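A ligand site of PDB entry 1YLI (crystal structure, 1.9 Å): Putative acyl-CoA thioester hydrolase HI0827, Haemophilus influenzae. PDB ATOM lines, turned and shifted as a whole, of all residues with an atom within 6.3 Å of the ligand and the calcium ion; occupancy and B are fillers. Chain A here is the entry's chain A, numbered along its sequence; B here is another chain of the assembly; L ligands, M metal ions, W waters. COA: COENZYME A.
N of Ser 90 sits at hydrogen-bond distance from O9A of the ligand, 2.8 Å away.
The side-chain hydroxyl (OG) of Ser 90 sits at hydrogen-bond distance from an oxygen (O9A) of the ligand (2.5 Å).
The backbone NH of Ser 91 is in hydrogen-bond range of an oxygen (O8A) of the ligand (3.0 Å).
The side-chain hydroxyl (OG) of Ser 91 lies within hydrogen-bond range of an oxygen (O8A) of the ligand (2.6 Å).
The side-chain hydroxyl (OG) of Ser 130 lies within hydrogen-bond range of an oxygen (O2A) of the ligand, at 2.6 Å.
N6A of the ligand lies within hydrogen-bond range of OD1 of Asn 67 of chain B (2.7 Å).
N of Arg 89 sits at hydrogen-bond distance from O8A of the ligand (2.8 Å).
An oxygen (O9A) of the ligand is in salt-bridge range of the guanidinium group (NE) of Arg 89 (3.7 Å).
O of Thr 60 is in hydrogen-bond range of N4P of the ligand (2.9 Å).
N8P of the ligand sits at hydrogen-bond distance from O of Phe 68 of chain B (3.0 Å).
O of Ile 69 of chain B sits at hydrogen-bond distance from N8P of the ligand, 3.4 Å away.
No residue comes within 4 Å of the calcium ion.
The nearest printed residue that does not touch the calcium ion is Val 61 (6.9 Å).
Residues that only touch the ligand: Gly 35 of chain B (3.3 Å), Pro 71 of chain B (3.3 Å), Gly 88 (3.4 Å), Lys 70 of chain B (3.5 Å), Val 122 (3.5 Å), Gly 128 (3.6 Å), Val 61 (3.7 Å), Val 59 (3.7 Å), Ala 62 (3.7 Å), Phe 34 of chain B (3.7 Å), Ile 33 of chain B (3.8 Å), Thr 120 (3.9 Å) and Val 114 of chain B (3.9 Å).
Hydrophobic or aromatic side chains that line the ligand: Val 59, Val 61, Ala 62, Val 122, Phe 68 of chain B, Pro 71 of chain B and Val 114 of chain B.
The calcium ion is bound by O4A of the ligand, water W3 and water W9.
The calcium ion has three donor atoms within binding distance.
NH2 of Arg 89 lies within hydrogen-bond range of OG of Ser 130 (2.9 Å).
The backbone NH (N) of Phe 68 of chain B is in hydrogen-bond range of the backbone carbonyl oxygen (O) of Val 61.
The backbone carbonyl oxygen (O) of Val 114 of chain B lies within hydrogen-bond range of the backbone NH (N) of Ile 69 of chain B.
N of Val 122 lies within hydrogen-bond range of O of Val 59.
The backbone carbonyl oxygen of Thr 120 lies within hydrogen-bond range of the backbone NH of Val 61 (2.9 Å).
N of Thr 120 is in hydrogen-bond range of O of Ala 62 (2.9 Å).
OG1 of Thr 120 is in hydrogen-bond range of NZ of Lys 93 (2.8 Å).
Water W6 lies within hydrogen-bond range of the backbone carbonyl oxygen of Gly 128 (2.5 Å) and an oxygen (O9P) of the ligand (2.7 Å).
Water W4 lies within hydrogen-bond range of an oxygen (O7A) of the ligand (2.8 Å) and the backbone NH (N) of Arg 89 (3.3 Å).
Water W5 lies within hydrogen-bond range of the backbone NH (N) of Ile 72 of chain B (2.8 Å), an oxygen (O5P) of the ligand (2.8 Å) and the backbone carbonyl oxygen (O) of Ile 33 of chain B (3.0 Å).
Water W7 bridges O9P of the ligand and O of Gly 128.
Water W2 bridges the backbone NH of Thr 60 (3.1 Å) and the backbone NH of Gly 35 of chain B (3.1 Å).
Water W8 lies within hydrogen-bond range of N of Ser 130 and O3A of the ligand.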
ATOM      1  N   VAL A  59      -6.188  10.036  18.954  1.00  0.00           N
ATOM      2  CA  VAL A  59      -5.479  10.681  20.070  1.00  0.00           C
ATOM      3  C   VAL A  59      -6.271  10.460  21.350  1.00  0.00           C
ATOM      4  O   VAL A  59      -7.472  10.173  21.301  1.00  0.00           O
ATOM      5  CB  VAL A  59      -5.328  12.194  19.866  1.00  0.00           C
ATOM      6  CG1 VAL A  59      -4.377  12.460  18.689  1.00  0.00           C
ATOM      7  CG2 VAL A  59      -6.708  12.853  19.676  1.00  0.00           C
ATOM      8  N   THR A  60      -5.589  10.624  22.488  1.00  0.00           N
ATOM      9  CA  THR A  60      -6.238  10.489  23.805  1.00  0.00           C
ATOM     10  C   THR A  60      -6.756  11.847  24.223  1.00  0.00           C
ATOM     11  O   THR A  60      -6.009  12.840  24.253  1.00  0.00           O
ATOM     12  CB  THR A  60      -5.256  10.009  24.897  1.00  0.00           C
ATOM     13  OG1 THR A  60      -4.582   8.845  24.438  1.00  0.00           O
ATOM     14  CG2 THR A  60      -6.000   9.691  26.189  1.00  0.00           C
ATOM     15  N   VAL A  61      -8.049  11.909  24.460  1.00  0.00           N
ATOM     16  CA  VAL A  61      -8.657  13.121  24.959  1.00  0.00           C
ATOM     17  C   VAL A  61      -8.849  13.090  26.490  1.00  0.00           C
ATOM     18  O   VAL A  61      -8.930  14.161  27.117  1.00  0.00           O
ATOM     19  CB  VAL A  61     -10.006  13.457  24.217  1.00  0.00           C
ATOM     20  CG1 VAL A  61     -11.099  12.421  24.557  1.00  0.00           C
ATOM     21  CG2 VAL A  61     -10.505  14.877  24.525  1.00  0.00           C
ATOM     22  N   ALA A  62      -8.956  11.907  27.090  1.00  0.00           N
ATOM     23  CA  ALA A  62      -9.291  11.817  28.527  1.00  0.00           C
ATOM     24  C   ALA A  62      -8.887  10.452  29.090  1.00  0.00           C
ATOM     25  O   ALA A  62      -8.842   9.494  28.352  1.00  0.00           O
ATOM     26  CB  ALA A  62     -10.848  12.034  28.790  1.00  0.00           C
ATOM     27  N   VAL A  87     -18.540   3.149  21.357  1.00  0.00           N
ATOM     28  CA  VAL A  87     -18.089   3.874  20.155  1.00  0.00           C
ATOM     29  C   VAL A  87     -19.077   4.989  19.851  1.00  0.00           C
ATOM     30  O   VAL A  87     -20.284   4.728  19.682  1.00  0.00           O
ATOM     31  CB  VAL A  87     -17.875   2.968  18.908  1.00  0.00           C
ATOM     32  CG1 VAL A  87     -17.344   3.792  17.742  1.00  0.00           C
ATOM     33  CG2 VAL A  87     -16.879   1.835  19.215  1.00  0.00           C
ATOM     34  N   GLY A  88     -18.588   6.217  19.803  1.00  0.00           N
ATOM     35  CA  GLY A  88     -19.449   7.382  19.495  1.00  0.00           C
ATOM     36  C   GLY A  88     -19.250   7.728  18.042  1.00  0.00           C
ATOM     37  O   GLY A  88     -19.029   6.846  17.216  1.00  0.00           O
ATOM     38  N   ARG A  89     -19.298   9.004  17.698  1.00  0.00           N
ATOM     39  CA  ARG A  89     -19.085   9.389  16.322  1.00  0.00           C
ATOM     40  C   ARG A  89     -17.576   9.370  16.042  1.00  0.00           C
ATOM     41  O   ARG A  89     -17.116   8.652  15.163  1.00  0.00           O
ATOM     42  CB  ARG A  89     -19.710  10.765  15.980  1.00  0.00           C
ATOM     43  CG  ARG A  89     -19.296  11.315  14.599  1.00  0.00           C
ATOM     44  CD  ARG A  89     -19.571  12.790  14.398  1.00  0.00           C
ATOM     45  NE  ARG A  89     -18.450  13.670  14.751  1.00  0.00           N
ATOM     46  CZ  ARG A  89     -17.570  14.199  13.880  1.00  0.00           C
ATOM     47  NH1 ARG A  89     -17.645  13.907  12.596  1.00  0.00           N
ATOM     48  NH2 ARG A  89     -16.622  15.003  14.298  1.00  0.00           N
ATOM     49  N   SER A  90     -16.808  10.102  16.837  1.00  0.00           N
ATOM     50  CA  SER A  90     -15.357  10.115  16.681  1.00  0.00           C
ATOM     51  C   SER A  90     -14.675   9.541  17.908  1.00  0.00           C
ATOM     52  O   SER A  90     -13.514   9.157  17.849  1.00  0.00           O
ATOM     53  CB  SER A  90     -14.840  11.541  16.412  1.00  0.00           C
ATOM     54  OG  SER A  90     -15.084  12.383  17.530  1.00  0.00           O
ATOM     55  N   SER A  91     -15.392   9.459  19.021  1.00  0.00           N
ATOM     56  CA  SER A  91     -14.774   8.953  20.243  1.00  0.00           C
ATOM     57  C   SER A  91     -14.949   7.439  20.443  1.00  0.00           C
ATOM     58  O   SER A  91     -15.927   6.838  19.983  1.00  0.00           O
ATOM     59  CB  SER A  91     -15.283   9.756  21.446  1.00  0.00           C
ATOM     60  OG  SER A  91     -16.697   9.624  21.590  1.00  0.00           O
ATOM     61  N   ILE A  92     -13.980   6.833  21.125  1.00  0.00           N
ATOM     62  CA  ILE A  92     -13.977   5.428  21.499  1.00  0.00           C
ATOM     63  C   ILE A  92     -13.521   5.333  22.961  1.00  0.00           C
ATOM     64  O   ILE A  92     -12.440   5.821  23.284  1.00  0.00           O
ATOM     65  CB  ILE A  92     -12.902   4.636  20.673  1.00  0.00           C
ATOM     66  CG1 ILE A  92     -13.168   4.809  19.194  1.00  0.00           C
ATOM     67  CG2 ILE A  92     -12.940   3.142  21.040  1.00  0.00           C
ATOM     68  CD1 ILE A  92     -11.929   4.687  18.351  1.00  0.00           C
ATOM     69  N   LYS A  93     -14.325   4.731  23.842  1.00  0.00           N
ATOM     70  CA  LYS A  93     -13.909   4.461  25.219  1.00  0.00           C
ATOM     71  C   LYS A  93     -13.315   3.054  25.353  1.00  0.00           C
ATOM     72  O   LYS A  93     -13.965   2.060  25.035  1.00  0.00           O
ATOM     73  CB  LYS A  93     -15.091   4.647  26.173  1.00  0.00           C
ATOM     74  CG  LYS A  93     -15.475   6.101  26.309  1.00  0.00           C
ATOM     75  CD  LYS A  93     -16.540   6.392  27.373  1.00  0.00           C
ATOM     76  CE  LYS A  93     -16.807   7.956  27.401  1.00  0.00           C
ATOM     77  NZ  LYS A  93     -15.624   8.808  27.911  1.00  0.00           N
ATOM     78  N   THR A 120     -10.442   7.533  26.879  1.00  0.00           N
ATOM     79  CA  THR A 120     -11.226   7.967  25.727  1.00  0.00           C
ATOM     80  C   THR A 120     -10.321   8.487  24.616  1.00  0.00           C
ATOM     81  O   THR A 120      -9.540   9.452  24.822  1.00  0.00           O
ATOM     82  CB  THR A 120     -12.211   9.063  26.137  1.00  0.00           C
ATOM     83  OG1 THR A 120     -12.941   8.584  27.262  1.00  0.00           O
ATOM     84  CG2 THR A 120     -13.177   9.383  24.965  1.00  0.00           C
ATOM     85  N   PHE A 121     -10.420   7.854  23.458  1.00  0.00           N
ATOM     86  CA  PHE A 121      -9.671   8.244  22.268  1.00  0.00           C
ATOM     87  C   PHE A 121     -10.605   8.962  21.278  1.00  0.00           C
ATOM     88  O   PHE A 121     -11.813   8.761  21.315  1.00  0.00           O
ATOM     89  CB  PHE A 121      -9.054   7.003  21.599  1.00  0.00           C
ATOM     90  CG  PHE A 121      -8.133   6.247  22.511  1.00  0.00           C
ATOM     91  CD1 PHE A 121      -6.788   6.651  22.665  1.00  0.00           C
ATOM     92  CD2 PHE A 121      -8.620   5.183  23.295  1.00  0.00           C
ATOM     93  CE1 PHE A 121      -5.938   5.995  23.574  1.00  0.00           C
ATOM     94  CE2 PHE A 121      -7.794   4.500  24.184  1.00  0.00           C
ATOM     95  CZ  PHE A 121      -6.434   4.899  24.322  1.00  0.00           C
ATOM     96  N   VAL A 122     -10.024   9.782  20.412  1.00  0.00           N
ATOM     97  CA  VAL A 122     -10.793  10.462  19.379  1.00  0.00           C
ATOM     98  C   VAL A 122     -10.093  10.182  18.039  1.00  0.00           C
ATOM     99  O   VAL A 122      -8.850  10.334  17.919  1.00  0.00           O
ATOM    100  CB  VAL A 122     -10.864  11.974  19.660  1.00  0.00           C
ATOM    101  CG1 VAL A 122     -11.612  12.728  18.509  1.00  0.00           C
ATOM    102  CG2 VAL A 122     -11.573  12.204  20.996  1.00  0.00           C
ATOM    103  N   VAL A 124      -8.957  11.187  14.588  1.00  0.00           N
ATOM    104  CA  VAL A 124      -8.571  12.488  14.025  1.00  0.00           C
ATOM    105  C   VAL A 124      -8.027  12.382  12.628  1.00  0.00           C
ATOM    106  O   VAL A 124      -7.462  11.364  12.235  1.00  0.00           O
ATOM    107  CB  VAL A 124      -7.598  13.290  14.933  1.00  0.00           C
ATOM    108  CG1 VAL A 124      -8.290  13.682  16.251  1.00  0.00           C
ATOM    109  CG2 VAL A 124      -6.323  12.491  15.222  1.00  0.00           C
ATOM    110  N   GLY A 128      -5.340  16.961  12.933  1.00  0.00           N
ATOM    111  CA  GLY A 128      -5.673  16.867  14.334  1.00  0.00           C
ATOM    112  C   GLY A 128      -7.130  17.100  14.690  1.00  0.00           C
ATOM    113  O   GLY A 128      -7.478  17.128  15.874  1.00  0.00           O
ATOM    114  N   ARG A 129      -7.982  17.261  13.672  1.00  0.00           N
ATOM    115  CA  ARG A 129      -9.420  17.475  13.892  1.00  0.00           C
ATOM    116  C   ARG A 129     -10.230  16.178  13.919  1.00  0.00           C
ATOM    117  O   ARG A 129      -9.914  15.245  13.208  1.00  0.00           O
ATOM    118  CB  ARG A 129      -9.990  18.464  12.855  1.00  0.00           C
ATOM    119  CG  ARG A 129      -9.380  19.889  13.024  1.00  0.00           C
ATOM    120  CD  ARG A 129     -10.011  20.893  12.072  1.00  0.00           C
ATOM    121  NE  ARG A 129      -8.981  21.688  11.401  1.00  0.00           N
ATOM    122  CZ  ARG A 129      -8.325  21.306  10.303  1.00  0.00           C
ATOM    123  NH1 ARG A 129      -8.587  20.119   9.719  1.00  0.00           N
ATOM    124  NH2 ARG A 129      -7.408  22.121   9.780  1.00  0.00           N
ATOM    125  N   SER A 130     -11.286  16.138  14.719  1.00  0.00           N
ATOM    126  CA  SER A 130     -12.074  14.910  14.847  1.00  0.00           C
ATOM    127  C   SER A 130     -12.666  14.439  13.503  1.00  0.00           C
ATOM    128  O   SER A 130     -13.040  15.255  12.648  1.00  0.00           O
ATOM    129  CB  SER A 130     -13.166  15.119  15.902  1.00  0.00           C
ATOM    130  OG  SER A 130     -14.172  15.976  15.402  1.00  0.00           O
ATOM    131  N   ARG A 131     -12.748  13.151  13.285  1.00  0.00           N
ATOM    132  CA  ARG A 131     -13.360  12.675  12.060  1.00  0.00           C
ATOM    133  C   ARG A 131     -14.337  11.578  12.441  1.00  0.00           C
ATOM    134  O   ARG A 131     -14.212  10.960  13.521  1.00  0.00           O
ATOM    135  CB  ARG A 131     -12.317  12.187  11.028  1.00  0.00           C
ATOM    136  CG  ARG A 131     -11.560  10.942  11.459  1.00  0.00           C
ATOM    137  CD  ARG A 131     -10.438  10.460  10.517  1.00  0.00           C
ATOM    138  NE  ARG A 131      -9.601   9.584  11.339  1.00  0.00           N
ATOM    139  CZ  ARG A 131      -9.852   8.297  11.593  1.00  0.00           C
ATOM    140  NH1 ARG A 131     -10.862   7.654  11.007  1.00  0.00           N
ATOM    141  NH2 ARG A 131      -9.056   7.639  12.429  1.00  0.00           N
ATOM    142  N   ILE B  33       3.134  12.908  19.663  1.00  0.00           N
ATOM    143  CA  ILE B  33       3.296  12.950  21.114  1.00  0.00           C
ATOM    144  C   ILE B  33       1.971  12.497  21.729  1.00  0.00           C
ATOM    145  O   ILE B  33       0.929  13.101  21.484  1.00  0.00           O
ATOM    146  CB  ILE B  33       3.662  14.373  21.582  1.00  0.00           C
ATOM    147  CG1 ILE B  33       5.062  14.773  21.055  1.00  0.00           C
ATOM    148  CG2 ILE B  33       3.517  14.524  23.131  1.00  0.00           C
ATOM    149  CD1 ILE B  33       6.217  13.800  21.486  1.00  0.00           C
ATOM    150  N   PHE B  34       2.009  11.431  22.520  1.00  0.00           N
ATOM    151  CA  PHE B  34       0.781  10.773  23.002  1.00  0.00           C
ATOM    152  C   PHE B  34       0.531  10.988  24.493  1.00  0.00           C
ATOM    153  O   PHE B  34       1.453  11.341  25.232  1.00  0.00           O
ATOM    154  CB  PHE B  34       0.784   9.269  22.604  1.00  0.00           C
ATOM    155  CG  PHE B  34       1.868   8.452  23.297  1.00  0.00           C
ATOM    156  CD1 PHE B  34       3.198   8.557  22.922  1.00  0.00           C
ATOM    157  CD2 PHE B  34       1.511   7.549  24.332  1.00  0.00           C
ATOM    158  CE1 PHE B  34       4.197   7.782  23.567  1.00  0.00           C
ATOM    159  CE2 PHE B  34       2.498   6.769  24.980  1.00  0.00           C
ATOM    160  CZ  PHE B  34       3.861   6.900  24.595  1.00  0.00           C
ATOM    161  N   GLY B  35      -0.729  10.790  24.921  1.00  0.00           N
ATOM    162  CA  GLY B  35      -1.160  10.994  26.314  1.00  0.00           C
ATOM    163  C   GLY B  35      -0.249  10.325  27.334  1.00  0.00           C
ATOM    164  O   GLY B  35       0.123  10.924  28.327  1.00  0.00           O
ATOM    165  N   GLY B  36       0.095   9.062  27.088  1.00  0.00           N
ATOM    166  CA  GLY B  36       0.928   8.308  28.003  1.00  0.00           C
ATOM    167  C   GLY B  36       2.278   8.947  28.315  1.00  0.00           C
ATOM    168  O   GLY B  36       2.734   8.889  29.444  1.00  0.00           O
ATOM    169  N   ILE B  38       2.928  12.189  28.265  1.00  0.00           N
ATOM    170  CA  ILE B  38       2.627  13.310  29.157  1.00  0.00           C
ATOM    171  C   ILE B  38       2.356  12.810  30.569  1.00  0.00           C
ATOM    172  O   ILE B  38       2.823  13.421  31.555  1.00  0.00           O
ATOM    173  CB  ILE B  38       1.416  14.153  28.627  1.00  0.00           C
ATOM    174  CG1 ILE B  38       1.784  14.763  27.277  1.00  0.00           C
ATOM    175  CG2 ILE B  38       1.003  15.298  29.608  1.00  0.00           C
ATOM    176  CD1 ILE B  38       2.968  15.739  27.349  1.00  0.00           C
ATOM    177  N   ASN B  67      -8.053  15.482  31.304  1.00  0.00           N
ATOM    178  CA  ASN B  67      -8.431  15.707  29.858  1.00  0.00           C
ATOM    179  C   ASN B  67      -7.225  16.330  29.198  1.00  0.00           C
ATOM    180  O   ASN B  67      -6.459  17.023  29.862  1.00  0.00           O
ATOM    181  CB  ASN B  67      -9.596  16.704  29.656  1.00  0.00           C
ATOM    182  CG  ASN B  67     -10.914  16.241  30.250  1.00  0.00           C
ATOM    183  OD1 ASN B  67     -11.460  15.207  29.847  1.00  0.00           O
ATOM    184  ND2 ASN B  67     -11.478  17.046  31.162  1.00  0.00           N
ATOM    185  N   PHE B  68      -7.027  16.092  27.898  1.00  0.00           N
ATOM    186  CA  PHE B  68      -5.897  16.701  27.148  1.00  0.00           C
ATOM    187  C   PHE B  68      -6.583  17.650  26.148  1.00  0.00           C
ATOM    188  O   PHE B  68      -7.263  17.201  25.224  1.00  0.00           O
ATOM    189  CB  PHE B  68      -5.029  15.623  26.446  1.00  0.00           C
ATOM    190  CG  PHE B  68      -4.443  14.597  27.400  1.00  0.00           C
ATOM    191  CD1 PHE B  68      -3.254  14.844  28.053  1.00  0.00           C
ATOM    192  CD2 PHE B  68      -5.127  13.431  27.706  1.00  0.00           C
ATOM    193  CE1 PHE B  68      -2.723  13.931  28.956  1.00  0.00           C
ATOM    194  CE2 PHE B  68      -4.624  12.518  28.628  1.00  0.00           C
ATOM    195  CZ  PHE B  68      -3.441  12.772  29.266  1.00  0.00           C
ATOM    196  N   ILE B  69      -6.396  18.950  26.328  1.00  0.00           N
ATOM    197  CA  ILE B  69      -7.166  19.895  25.528  1.00  0.00           C
ATOM    198  C   ILE B  69      -6.568  20.256  24.160  1.00  0.00           C
ATOM    199  O   ILE B  69      -7.314  20.616  23.250  1.00  0.00           O
ATOM    200  CB  ILE B  69      -7.509  21.201  26.281  1.00  0.00           C
ATOM    201  CG1 ILE B  69      -6.233  21.990  26.646  1.00  0.00           C
ATOM    202  CG2 ILE B  69      -8.407  20.920  27.491  1.00  0.00           C
ATOM    203  CD1 ILE B  69      -6.474  23.543  26.665  1.00  0.00           C
ATOM    204  N   LYS B  70      -5.247  20.130  24.025  1.00  0.00           N
ATOM    205  CA  LYS B  70      -4.551  20.559  22.820  1.00  0.00           C
ATOM    206  C   LYS B  70      -3.362  19.619  22.587  1.00  0.00           C
ATOM    207  O   LYS B  70      -2.765  19.159  23.549  1.00  0.00           O
ATOM    208  CB  LYS B  70      -4.062  22.012  22.962  1.00  0.00           C
ATOM    209  CG  LYS B  70      -5.150  23.073  22.702  1.00  0.00           C
ATOM    210  CD  LYS B  70      -4.632  24.529  22.840  1.00  0.00           C
ATOM    211  CE  LYS B  70      -3.671  24.921  21.645  1.00  0.00           C
ATOM    212  NZ  LYS B  70      -3.511  26.434  21.411  1.00  0.00           N
ATOM    213  N   PRO B  71      -3.055  19.323  21.300  1.00  0.00           N
ATOM    214  CA  PRO B  71      -1.936  18.426  20.981  1.00  0.00           C
ATOM    215  C   PRO B  71      -0.563  19.068  21.224  1.00  0.00           C
ATOM    216  O   PRO B  71      -0.489  20.292  21.411  1.00  0.00           O
ATOM    217  CB  PRO B  71      -2.136  18.128  19.503  1.00  0.00           C
ATOM    218  CG  PRO B  71      -2.945  19.302  18.977  1.00  0.00           C
ATOM    219  CD  PRO B  71      -3.759  19.776  20.084  1.00  0.00           C
ATOM    220  N   ILE B  72       0.489  18.264  21.266  1.00  0.00           N
ATOM    221  CA  ILE B  72       1.850  18.773  21.390  1.00  0.00           C
ATOM    222  C   ILE B  72       2.607  18.235  20.172  1.00  0.00           C
ATOM    223  O   ILE B  72       2.348  17.072  19.764  1.00  0.00           O
ATOM    224  CB  ILE B  72       2.473  18.257  22.686  1.00  0.00           C
ATOM    225  CG1 ILE B  72       1.584  18.672  23.879  1.00  0.00           C
ATOM    226  CG2 ILE B  72       3.929  18.774  22.863  1.00  0.00           C
ATOM    227  CD1 ILE B  72       1.991  17.965  25.202  1.00  0.00           C
ATOM    228  N   VAL B 114      -1.919  22.086  28.596  1.00  0.00           N
ATOM    229  CA  VAL B 114      -2.415  20.850  27.993  1.00  0.00           C
ATOM    230  C   VAL B 114      -3.319  20.072  28.921  1.00  0.00           C
ATOM    231  O   VAL B 114      -4.427  19.653  28.544  1.00  0.00           O
ATOM    232  CB  VAL B 114      -1.218  19.961  27.605  1.00  0.00           C
ATOM    233  CG1 VAL B 114      -1.640  18.569  27.167  1.00  0.00           C
ATOM    234  CG2 VAL B 114      -0.522  20.636  26.484  1.00  0.00           C
HETATM  235  N1A COA L   1     -13.970  13.549  27.466  1.00  0.00           N
HETATM  236  C2A COA L   1     -14.588  12.591  26.703  1.00  0.00           C
HETATM  237  N3A COA L   1     -14.938  12.884  25.422  1.00  0.00           N
HETATM  238  C4A COA L   1     -14.639  14.106  24.921  1.00  0.00           C
HETATM  239  C5A COA L   1     -14.030  15.072  25.692  1.00  0.00           C
HETATM  240  C6A COA L   1     -13.661  14.779  26.985  1.00  0.00           C
HETATM  241  N6A COA L   1     -13.180  15.700  27.809  1.00  0.00           N
HETATM  242  N7A COA L   1     -13.890  16.187  24.956  1.00  0.00           N
HETATM  243  C8A COA L   1     -14.403  15.926  23.728  1.00  0.00           C
HETATM  244  N9A COA L   1     -14.880  14.638  23.698  1.00  0.00           N
HETATM  245  C1B COA L   1     -15.501  13.944  22.559  1.00  0.00           C
HETATM  246  C2B COA L   1     -16.702  14.676  21.991  1.00  0.00           C
HETATM  247  O2B COA L   1     -17.891  14.518  22.728  1.00  0.00           O
HETATM  248  C3B COA L   1     -16.759  14.056  20.607  1.00  0.00           C
HETATM  249  O3B COA L   1     -17.289  12.748  20.696  1.00  0.00           O
HETATM  250  P3B COA L   1     -18.080  12.019  19.498  1.00  0.00           P
HETATM  251  O7A COA L   1     -19.498  12.562  19.587  1.00  0.00           O
HETATM  252  O8A COA L   1     -18.098  10.544  19.663  1.00  0.00           O
HETATM  253  O9A COA L   1     -17.552  12.439  18.155  1.00  0.00           O
HETATM  254  C4B COA L   1     -15.287  13.889  20.273  1.00  0.00           C
HETATM  255  O4B COA L   1     -14.599  13.922  21.500  1.00  0.00           O
HETATM  256  C5B COA L   1     -14.778  14.990  19.341  1.00  0.00           C
HETATM  257  O5B COA L   1     -15.206  16.238  19.869  1.00  0.00           O
HETATM  258  P1A COA L   1     -15.125  17.510  18.929  1.00  0.00           P
HETATM  259  O1A COA L   1     -16.096  18.556  19.411  1.00  0.00           O
HETATM  260  O2A COA L   1     -15.318  17.108  17.485  1.00  0.00           O
HETATM  261  O3A COA L   1     -13.582  18.004  18.940  1.00  0.00           O
HETATM  262  P2A COA L   1     -13.006  18.985  20.045  1.00  0.00           P
HETATM  263  O4A COA L   1     -13.894  18.697  21.248  1.00  0.00           O
HETATM  264  O5A COA L   1     -13.041  20.434  19.608  1.00  0.00           O
HETATM  265  O6A COA L   1     -11.508  18.434  20.200  1.00  0.00           O
HETATM  266  CBP COA L   1      -9.729  16.874  20.323  1.00  0.00           C
HETATM  267  CCP COA L   1     -11.226  17.077  20.502  1.00  0.00           C
HETATM  268  CDP COA L   1      -9.370  15.518  20.955  1.00  0.00           C
HETATM  269  CEP COA L   1      -9.511  16.876  18.816  1.00  0.00           C
HETATM  270  CAP COA L   1      -8.954  18.011  21.019  1.00  0.00           C
HETATM  271  OAP COA L   1      -9.463  18.090  22.337  1.00  0.00           O
HETATM  272  C9P COA L   1      -7.470  17.730  21.060  1.00  0.00           C
HETATM  273  O9P COA L   1      -6.737  17.786  19.855  1.00  0.00           O
HETATM  274  N8P COA L   1      -6.921  17.386  22.231  1.00  0.00           N
HETATM  275  C7P COA L   1      -5.539  16.921  22.363  1.00  0.00           C
HETATM  276  C6P COA L   1      -5.421  15.453  21.988  1.00  0.00           C
HETATM  277  C5P COA L   1      -3.991  14.984  22.078  1.00  0.00           C
HETATM  278  O5P COA L   1      -3.179  15.335  21.214  1.00  0.00           O
HETATM  279  N4P COA L   1      -3.725  14.146  23.088  1.00  0.00           N
HETATM  280  C3P COA L   1      -2.432  13.508  23.250  1.00  0.00           C
HETATM  281  C2P COA L   1      -1.777  13.926  24.553  1.00  0.00           C
HETATM  282  S1P COA L   1      -1.382  15.682  24.534  1.00  0.00           S
HETATM  283 CA    CA M   1     -14.854  20.028  22.958  1.00  0.00          CA
HETATM  284  O   HOH W   1     -18.486  17.293  23.938  1.00  0.00           O
HETATM  285  O   HOH W   2      -2.502  10.542  22.377  1.00  0.00           O
HETATM  286  O   HOH W   3     -13.336  19.054  24.540  1.00  0.00           O
HETATM  287  O   HOH W   4     -21.553  10.727  19.344  1.00  0.00           O
HETATM  288  O   HOH W   5      -0.453  15.691  20.827  1.00  0.00           O
HETATM  289  O   HOH W   6      -5.975  16.278  17.688  1.00  0.00           O
HETATM  290  O   HOH W   7      -7.277  19.710  17.623  1.00  0.00           O
HETATM  291  O   HOH W   8     -11.872  18.527  16.371  1.00  0.00           O
HETATM  292  O   HOH W   9     -17.152  19.599  21.768  1.00  0.00           O
